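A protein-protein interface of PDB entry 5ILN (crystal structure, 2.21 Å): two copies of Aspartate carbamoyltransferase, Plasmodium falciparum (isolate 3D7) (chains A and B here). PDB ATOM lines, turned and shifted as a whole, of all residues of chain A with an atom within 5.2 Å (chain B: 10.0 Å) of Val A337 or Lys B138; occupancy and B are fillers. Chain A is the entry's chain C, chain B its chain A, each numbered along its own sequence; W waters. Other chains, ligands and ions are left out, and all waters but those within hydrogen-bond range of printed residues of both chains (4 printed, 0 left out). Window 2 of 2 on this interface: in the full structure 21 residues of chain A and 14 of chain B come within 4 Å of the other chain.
The backbone carbonyl oxygen (O) of Ser B133 sits at hydrogen-bond distance from the backbone NH (N) of Ser A107, at 3.0 Å. The side-chain carboxylate (OD1) of Asp B144 is in salt-bridge range of the guanidinium group (NH2) of Arg A336, 2.8 Å away.
The side-chain carboxylate of Asp B130 lies close to the backbone NH of Asn B132, at 3.5 Å. O of Asp B130 is in hydrogen-bond range of OG of Ser B133 (3.1 Å). The side-chain sulfur (SD) of Met B131 sits close to the side-chain amide oxygen (OD1) of Asn B132 (3.0 Å). The side-chain amino group (NZ) of Lys B138 sits at hydrogen-bond distance from the side-chain hydroxyl (OG) of Ser B135, at 3.3 Å. The guanidinium group (NH2) of Arg A295 is in salt-bridge range of the side-chain carboxylate (OE2) of Glu A299. N of Val A337 is in hydrogen-bond range of OE1 of Glu A339 (3.0 Å).
Among the printed residues, merely in contact across the chains: Pro A106 with Asn B132, Pro A106 with Ser B133, Pro A106 with Thr B134, Pro A106 with Tyr B137, Pro A106 with Lys B138, Ser A107 with Thr B134, Ser A107 with Ser B135, Arg A295 with Lys B138, Pro A335 with Glu B140 and Val A337 with Lys B138.
Val A337 touches just one residue of chain B: Lys B138. Of chain A, only Pro A106, Arg A295 and Val A337 come within 4 Å of Lys B138. Of chain B, only Asn B132 (3.4 Å), Ser B133 (3.5 Å), Thr B134 (3.4 Å), Tyr B137 (3.97 Å) and Lys B138 (3.8 Å) come within 4 Å of Pro A106. Of chain B, only Glu B140 (3.7 Å) comes within 4 Å of Pro A335. Asn A338 touches none of the printed residues of chain B. Of the printed residues of chain A, Ser B133 touches Pro A106 (3.5 Å) and Ser A107 (3.0 Å). Of the printed residues of chain B, Arg A295 touches Lys B138. Glu A299 touches none of the printed residues of chain B. The nearest residue of chain B that does not touch Val A337 is Gly B139 (5.1 Å). The nearest residue of chain A that does not touch Lys B138 is Pro A335 (4.2 Å).
Of the 13 printed residues of chain B, 8 touch a printed residue of chain A. Hydrophobic or aromatic side chains of chain B that line the printed part of chain A: Tyr B137. Printed residues of chain A that touch a printed residue of chain B: Pro A106, Ser A107, Arg A295, Pro A335, Arg A336 and Val A337. Among the printed residues, 12 pairs touch across the chains. Among the printed residues, Asp or Glu carboxylates within 4 Å of a Lys or Arg side-chain nitrogen of the other chain: Arg A336 with Asp B144 (2.8 Å).
No position is printed for both chains.
Water W4 lies within hydrogen-bond range of the backbone carbonyl oxygen of Pro A106 (2.7 Å), the guanidinium group of Arg A159 (2.8 Å) and the side-chain amino group of Lys B138 (3.2 Å). Water W3 lies within hydrogen-bond range of OD2 of Asp B144, O of Arg A336 and N of Thr B141. Water W1 lies within hydrogen-bond range of the side-chain carboxylate of Asp B144 (2.8 Å), the side-chain carboxylate of Glu B140 (2.8 Å) and the backbone NH of Arg A336 (2.9 Å). Water W2 bridges O of Ser B133 and N of Ser A107.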
ATOM      1  N   PRO A 106      -1.010   3.335 -18.393  1.00  0.00           N
ATOM      2  CA  PRO A 106       0.311   2.785 -18.059  1.00  0.00           C
ATOM      3  C   PRO A 106       0.312   1.262 -17.842  1.00  0.00           C
ATOM      4  O   PRO A 106      -0.652   0.678 -17.296  1.00  0.00           O
ATOM      5  CB  PRO A 106       0.690   3.574 -16.795  1.00  0.00           C
ATOM      6  CG  PRO A 106      -0.051   4.871 -16.904  1.00  0.00           C
ATOM      7  CD  PRO A 106      -1.362   4.460 -17.483  1.00  0.00           C
ATOM      8  N   SER A 107       1.345   0.628 -18.324  1.00  0.00           N
ATOM      9  CA  SER A 107       1.523  -0.818 -18.101  1.00  0.00           C
ATOM     10  C   SER A 107       2.957  -1.309 -18.235  1.00  0.00           C
ATOM     11  O   SER A 107       3.636  -0.906 -19.131  1.00  0.00           O
ATOM     12  CB  SER A 107       0.686  -1.586 -19.084  1.00  0.00           C
ATOM     13  OG  SER A 107       0.925  -2.996 -18.907  1.00  0.00           O
ATOM     14  N   ARG A 159      -5.646  -2.021 -24.144  1.00  0.00           N
ATOM     15  CA  ARG A 159      -5.856  -1.510 -22.837  1.00  0.00           C
ATOM     16  C   ARG A 159      -6.296  -0.060 -22.918  1.00  0.00           C
ATOM     17  O   ARG A 159      -5.566   0.761 -23.487  1.00  0.00           O
ATOM     18  CB  ARG A 159      -4.586  -1.591 -21.964  1.00  0.00           C
ATOM     19  CG  ARG A 159      -4.893  -0.984 -20.634  1.00  0.00           C
ATOM     20  CD  ARG A 159      -3.870  -1.154 -19.543  1.00  0.00           C
ATOM     21  NE  ARG A 159      -3.885  -2.468 -18.992  1.00  0.00           N
ATOM     22  CZ  ARG A 159      -3.135  -2.879 -17.994  1.00  0.00           C
ATOM     23  NH1 ARG A 159      -3.186  -4.158 -17.647  1.00  0.00           N
ATOM     24  NH2 ARG A 159      -2.336  -2.035 -17.361  1.00  0.00           N
ATOM     25  N   ARG A 295      -3.559  -3.704  -5.048  1.00  0.00           N
ATOM     26  CA  ARG A 295      -3.175  -2.279  -4.812  1.00  0.00           C
ATOM     27  C   ARG A 295      -4.383  -1.356  -4.540  1.00  0.00           C
ATOM     28  O   ARG A 295      -5.420  -1.461  -5.172  1.00  0.00           O
ATOM     29  CB  ARG A 295      -2.268  -1.794  -5.958  1.00  0.00           C
ATOM     30  CG  ARG A 295      -1.841  -0.342  -5.951  1.00  0.00           C
ATOM     31  CD  ARG A 295      -1.006  -0.017  -7.173  1.00  0.00           C
ATOM     32  NE  ARG A 295      -1.753   0.017  -8.448  1.00  0.00           N
ATOM     33  CZ  ARG A 295      -2.440   1.068  -8.945  1.00  0.00           C
ATOM     34  NH1 ARG A 295      -2.582   2.245  -8.317  1.00  0.00           N
ATOM     35  NH2 ARG A 295      -3.056   0.942 -10.113  1.00  0.00           N
ATOM     36  N   GLU A 299      -5.313   6.642  -7.585  1.00  0.00           N
ATOM     37  CA  GLU A 299      -5.856   7.428  -8.721  1.00  0.00           C
ATOM     38  C   GLU A 299      -7.328   7.505  -8.715  1.00  0.00           C
ATOM     39  O   GLU A 299      -7.883   8.189  -9.507  1.00  0.00           O
ATOM     40  CB  GLU A 299      -5.398   6.872 -10.123  1.00  0.00           C
ATOM     41  CG  GLU A 299      -5.744   5.403 -10.415  1.00  0.00           C
ATOM     42  CD  GLU A 299      -4.671   4.426  -9.958  1.00  0.00           C
ATOM     43  OE1 GLU A 299      -3.882   4.762  -9.044  1.00  0.00           O
ATOM     44  OE2 GLU A 299      -4.664   3.276 -10.462  1.00  0.00           O
ATOM     45  N   LYS A 311      -5.012   3.017   2.612  1.00  0.00           N
ATOM     46  CA  LYS A 311      -3.698   2.626   2.132  1.00  0.00           C
ATOM     47  C   LYS A 311      -3.032   1.781   3.122  1.00  0.00           C
ATOM     48  O   LYS A 311      -2.360   0.830   2.788  1.00  0.00           O
ATOM     49  CB  LYS A 311      -2.847   3.897   1.927  1.00  0.00           C
ATOM     50  CG  LYS A 311      -1.430   3.802   1.325  1.00  0.00           C
ATOM     51  CD  LYS A 311      -0.651   5.129   1.551  1.00  0.00           C
ATOM     52  CE  LYS A 311       0.536   5.376   0.596  1.00  0.00           C
ATOM     53  NZ  LYS A 311       1.289   4.121   0.338  1.00  0.00           N
ATOM     54  N   PRO A 335       1.406  -3.899 -10.200  1.00  0.00           N
ATOM     55  CA  PRO A 335       2.408  -3.654  -9.160  1.00  0.00           C
ATOM     56  C   PRO A 335       1.874  -3.403  -7.751  1.00  0.00           C
ATOM     57  O   PRO A 335       0.674  -3.036  -7.535  1.00  0.00           O
ATOM     58  CB  PRO A 335       3.011  -2.409  -9.663  1.00  0.00           C
ATOM     59  CG  PRO A 335       1.831  -1.614 -10.090  1.00  0.00           C
ATOM     60  CD  PRO A 335       0.917  -2.599 -10.725  1.00  0.00           C
ATOM     61  N   ARG A 336       2.739  -3.690  -6.808  1.00  0.00           N
ATOM     62  CA  ARG A 336       2.457  -3.382  -5.395  1.00  0.00           C
ATOM     63  C   ARG A 336       3.085  -1.995  -4.986  1.00  0.00           C
ATOM     64  O   ARG A 336       4.075  -1.515  -5.606  1.00  0.00           O
ATOM     65  CB  ARG A 336       2.982  -4.505  -4.505  1.00  0.00           C
ATOM     66  CG  ARG A 336       4.446  -4.654  -4.571  1.00  0.00           C
ATOM     67  CD  ARG A 336       5.047  -5.260  -3.329  1.00  0.00           C
ATOM     68  NE  ARG A 336       6.373  -5.679  -3.751  1.00  0.00           N
ATOM     69  CZ  ARG A 336       7.127  -6.570  -3.148  1.00  0.00           C
ATOM     70  NH1 ARG A 336       6.731  -7.114  -1.993  1.00  0.00           N
ATOM     71  NH2 ARG A 336       8.304  -6.902  -3.709  1.00  0.00           N
ATOM     72  N   VAL A 337       2.487  -1.354  -3.994  1.00  0.00           N
ATOM     73  CA  VAL A 337       3.117  -0.208  -3.330  1.00  0.00           C
ATOM     74  C   VAL A 337       3.558  -0.804  -1.940  1.00  0.00           C
ATOM     75  O   VAL A 337       4.454  -1.590  -1.869  1.00  0.00           O
ATOM     76  CB  VAL A 337       2.134   1.030  -3.284  1.00  0.00           C
ATOM     77  CG1 VAL A 337       2.714   2.255  -2.553  1.00  0.00           C
ATOM     78  CG2 VAL A 337       1.675   1.491  -4.680  1.00  0.00           C
ATOM     79  N   ASN A 338       2.848  -0.506  -0.848  1.00  0.00           N
ATOM     80  CA  ASN A 338       3.215  -0.933   0.512  1.00  0.00           C
ATOM     81  C   ASN A 338       2.441  -2.176   1.045  1.00  0.00           C
ATOM     82  O   ASN A 338       2.822  -2.729   2.046  1.00  0.00           O
ATOM     83  CB  ASN A 338       3.056   0.235   1.467  1.00  0.00           C
ATOM     84  CG  ASN A 338       1.590   0.527   1.798  1.00  0.00           C
ATOM     85  OD1 ASN A 338       1.250   0.639   2.966  1.00  0.00           O
ATOM     86  ND2 ASN A 338       0.737   0.692   0.808  1.00  0.00           N
ATOM     87  N   GLU A 339       1.393  -2.617   0.342  1.00  0.00           N
ATOM     88  CA  GLU A 339       0.558  -3.713   0.796  1.00  0.00           C
ATOM     89  C   GLU A 339       1.208  -5.088   1.025  1.00  0.00           C
ATOM     90  O   GLU A 339       0.603  -5.922   1.621  1.00  0.00           O
ATOM     91  CB  GLU A 339      -0.722  -3.821  -0.044  1.00  0.00           C
ATOM     92  CG  GLU A 339      -0.440  -4.327  -1.458  1.00  0.00           C
ATOM     93  CD  GLU A 339      -0.135  -3.230  -2.466  1.00  0.00           C
ATOM     94  OE1 GLU A 339       0.314  -2.146  -2.066  1.00  0.00           O
ATOM     95  OE2 GLU A 339      -0.305  -3.471  -3.667  1.00  0.00           O
ATOM     96  N   ILE A 340       2.400  -5.346   0.556  1.00  0.00           N
ATOM     97  CA  ILE A 340       3.107  -6.568   0.959  1.00  0.00           C
ATOM     98  C   ILE A 340       4.512  -6.114   1.264  1.00  0.00           C
ATOM     99  O   ILE A 340       5.180  -5.610   0.385  1.00  0.00           O
ATOM    100  CB  ILE A 340       3.175  -7.629  -0.159  1.00  0.00           C
ATOM    101  CG1 ILE A 340       1.786  -8.115  -0.539  1.00  0.00           C
ATOM    102  CG2 ILE A 340       4.071  -8.795   0.240  1.00  0.00           C
ATOM    103  CD1 ILE A 340       1.770  -8.992  -1.789  1.00  0.00           C
ATOM    104  N   ASP B 130       9.828   5.954 -21.708  1.00  0.00           N
ATOM    105  CA  ASP B 130       9.703   6.742 -20.477  1.00  0.00           C
ATOM    106  C   ASP B 130       8.802   6.172 -19.442  1.00  0.00           C
ATOM    107  O   ASP B 130       7.780   5.621 -19.778  1.00  0.00           O
ATOM    108  CB  ASP B 130       9.154   8.176 -20.683  1.00  0.00           C
ATOM    109  CG  ASP B 130       7.816   8.183 -21.258  1.00  0.00           C
ATOM    110  OD1 ASP B 130       7.732   7.467 -22.250  1.00  0.00           O
ATOM    111  OD2 ASP B 130       6.911   8.872 -20.730  1.00  0.00           O
ATOM    112  N   MET B 131       9.150   6.561 -18.214  1.00  0.00           N
ATOM    113  CA  MET B 131       8.536   6.292 -16.943  1.00  0.00           C
ATOM    114  C   MET B 131       6.966   6.320 -17.027  1.00  0.00           C
ATOM    115  O   MET B 131       6.306   5.409 -16.550  1.00  0.00           O
ATOM    116  CB  MET B 131       9.206   7.283 -15.900  1.00  0.00           C
ATOM    117  CG  MET B 131       8.739   7.390 -14.426  1.00  0.00           C
ATOM    118  SD  MET B 131       7.099   8.146 -13.984  1.00  0.00           S
ATOM    119  CE  MET B 131       7.309   8.539 -12.206  1.00  0.00           C
ATOM    120  N   ASN B 132       6.373   7.283 -17.691  1.00  0.00           N
ATOM    121  CA  ASN B 132       4.898   7.469 -17.663  1.00  0.00           C
ATOM    122  C   ASN B 132       3.979   6.457 -18.336  1.00  0.00           C
ATOM    123  O   ASN B 132       2.838   6.315 -17.895  1.00  0.00           O
ATOM    124  CB  ASN B 132       4.542   8.851 -18.159  1.00  0.00           C
ATOM    125  CG  ASN B 132       5.023   9.928 -17.176  1.00  0.00           C
ATOM    126  OD1 ASN B 132       5.511   9.621 -16.045  1.00  0.00           O
ATOM    127  ND2 ASN B 132       4.909  11.188 -17.591  1.00  0.00           N
ATOM    128  N   SER B 133       4.520   5.706 -19.302  1.00  0.00           N
ATOM    129  CA  SER B 133       3.825   4.685 -20.034  1.00  0.00           C
ATOM    130  C   SER B 133       3.903   3.310 -19.340  1.00  0.00           C
ATOM    131  O   SER B 133       3.331   2.325 -19.762  1.00  0.00           O
ATOM    132  CB  SER B 133       4.438   4.612 -21.447  1.00  0.00           C
ATOM    133  OG  SER B 133       5.745   4.030 -21.416  1.00  0.00           O
ATOM    134  N   THR B 134       4.513   3.323 -18.198  1.00  0.00           N
ATOM    135  CA  THR B 134       5.024   2.201 -17.463  1.00  0.00           C
ATOM    136  C   THR B 134       4.359   2.181 -16.032  1.00  0.00           C
ATOM    137  O   THR B 134       3.814   3.186 -15.554  1.00  0.00           O
ATOM    138  CB  THR B 134       6.554   2.472 -17.403  1.00  0.00           C
ATOM    139  OG1 THR B 134       7.266   1.746 -18.448  1.00  0.00           O
ATOM    140  CG2 THR B 134       7.047   2.218 -16.156  1.00  0.00           C
ATOM    141  N   SER B 135       4.394   1.022 -15.382  1.00  0.00           N
ATOM    142  CA  SER B 135       3.914   0.885 -14.002  1.00  0.00           C
ATOM    143  C   SER B 135       4.768   1.618 -12.943  1.00  0.00           C
ATOM    144  O   SER B 135       4.314   1.818 -11.795  1.00  0.00           O
ATOM    145  CB  SER B 135       3.586  -0.579 -13.647  1.00  0.00           C
ATOM    146  OG  SER B 135       2.278  -0.878 -14.201  1.00  0.00           O
ATOM    147  N   PHE B 136       5.982   2.075 -13.313  1.00  0.00           N
ATOM    148  CA  PHE B 136       6.632   3.159 -12.494  1.00  0.00           C
ATOM    149  C   PHE B 136       5.633   4.275 -12.189  1.00  0.00           C
ATOM    150  O   PHE B 136       5.608   4.725 -11.083  1.00  0.00           O
ATOM    151  CB  PHE B 136       7.980   3.719 -13.071  1.00  0.00           C
ATOM    152  CG  PHE B 136       9.023   2.676 -13.262  1.00  0.00           C
ATOM    153  CD1 PHE B 136       9.390   1.857 -12.209  1.00  0.00           C
ATOM    154  CD2 PHE B 136       9.658   2.505 -14.510  1.00  0.00           C
ATOM    155  CE1 PHE B 136      10.351   0.868 -12.390  1.00  0.00           C
ATOM    156  CE2 PHE B 136      10.589   1.533 -14.721  1.00  0.00           C
ATOM    157  CZ  PHE B 136      10.943   0.722 -13.649  1.00  0.00           C
ATOM    158  N   TYR B 137       4.798   4.673 -13.166  1.00  0.00           N
ATOM    159  CA  TYR B 137       3.806   5.742 -12.979  1.00  0.00           C
ATOM    160  C   TYR B 137       3.008   5.624 -11.721  1.00  0.00           C
ATOM    161  O   TYR B 137       2.604   6.616 -11.189  1.00  0.00           O
ATOM    162  CB  TYR B 137       2.800   5.814 -14.122  1.00  0.00           C
ATOM    163  CG  TYR B 137       2.040   7.103 -14.077  1.00  0.00           C
ATOM    164  CD1 TYR B 137       2.689   8.351 -14.328  1.00  0.00           C
ATOM    165  CD2 TYR B 137       0.696   7.116 -13.710  1.00  0.00           C
ATOM    166  CE1 TYR B 137       1.997   9.546 -14.233  1.00  0.00           C
ATOM    167  CE2 TYR B 137       0.002   8.299 -13.617  1.00  0.00           C
ATOM    168  CZ  TYR B 137       0.624   9.509 -13.889  1.00  0.00           C
ATOM    169  OH  TYR B 137      -0.155  10.668 -13.778  1.00  0.00           O
ATOM    170  N   LYS B 138       2.730   4.393 -11.311  1.00  0.00           N
ATOM    171  CA  LYS B 138       1.895   4.061 -10.143  1.00  0.00           C
ATOM    172  C   LYS B 138       2.730   3.767  -8.885  1.00  0.00           C
ATOM    173  O   LYS B 138       2.175   3.334  -7.879  1.00  0.00           O
ATOM    174  CB  LYS B 138       1.099   2.804 -10.491  1.00  0.00           C
ATOM    175  CG  LYS B 138       0.314   2.827 -11.828  1.00  0.00           C
ATOM    176  CD  LYS B 138      -0.281   1.443 -12.091  1.00  0.00           C
ATOM    177  CE  LYS B 138      -0.974   1.234 -13.421  1.00  0.00           C
ATOM    178  NZ  LYS B 138      -0.923  -0.249 -13.651  1.00  0.00           N
ATOM    179  N   GLY B 139       4.064   3.924  -9.010  1.00  0.00           N
ATOM    180  CA  GLY B 139       5.031   3.782  -7.905  1.00  0.00           C
ATOM    181  C   GLY B 139       5.724   2.457  -7.765  1.00  0.00           C
ATOM    182  O   GLY B 139       6.253   2.172  -6.702  1.00  0.00           O
ATOM    183  N   GLU B 140       5.750   1.615  -8.811  1.00  0.00           N
ATOM    184  CA  GLU B 140       6.451   0.341  -8.703  1.00  0.00           C
ATOM    185  C   GLU B 140       7.917   0.628  -8.447  1.00  0.00           C
ATOM    186  O   GLU B 140       8.399   1.522  -9.047  1.00  0.00           O
ATOM    187  CB  GLU B 140       6.355  -0.478 -10.003  1.00  0.00           C
ATOM    188  CG  GLU B 140       7.101  -1.818  -9.968  1.00  0.00           C
ATOM    189  CD  GLU B 140       6.517  -2.877 -10.894  1.00  0.00           C
ATOM    190  OE1 GLU B 140       6.002  -2.543 -12.006  1.00  0.00           O
ATOM    191  OE2 GLU B 140       6.543  -4.084 -10.527  1.00  0.00           O
ATOM    192  N   THR B 141       8.602  -0.181  -7.619  1.00  0.00           N
ATOM    193  CA  THR B 141       9.995  -0.065  -7.391  1.00  0.00           C
ATOM    194  C   THR B 141      10.829  -0.575  -8.594  1.00  0.00           C
ATOM    195  O   THR B 141      10.405  -1.386  -9.390  1.00  0.00           O
ATOM    196  CB  THR B 141      10.436  -0.829  -6.153  1.00  0.00           C
ATOM    197  OG1 THR B 141      10.158  -2.225  -6.319  1.00  0.00           O
ATOM    198  CG2 THR B 141       9.681  -0.319  -4.845  1.00  0.00           C
ATOM    199  N   ASP B 144      11.440  -4.523  -8.278  1.00  0.00           N
ATOM    200  CA  ASP B 144      10.291  -5.330  -8.692  1.00  0.00           C
ATOM    201  C   ASP B 144      10.260  -5.329 -10.195  1.00  0.00           C
ATOM    202  O   ASP B 144      10.118  -6.368 -10.792  1.00  0.00           O
ATOM    203  CB  ASP B 144       8.919  -4.729  -8.200  1.00  0.00           C
ATOM    204  CG  ASP B 144       8.598  -5.007  -6.698  1.00  0.00           C
ATOM    205  OD1 ASP B 144       9.356  -5.681  -6.028  1.00  0.00           O
ATOM    206  OD2 ASP B 144       7.515  -4.543  -6.186  1.00  0.00           O
HETATM  207  O   HOH W   1       5.422  -4.041  -7.939  1.00  0.00           O
HETATM  208  O   HOH W   2       1.289   1.497 -21.482  1.00  0.00           O
HETATM  209  O   HOH W   3       6.723  -1.931  -6.138  1.00  0.00           O
HETATM  210  O   HOH W   4      -3.010   0.375 -16.052  1.00  0.00           O
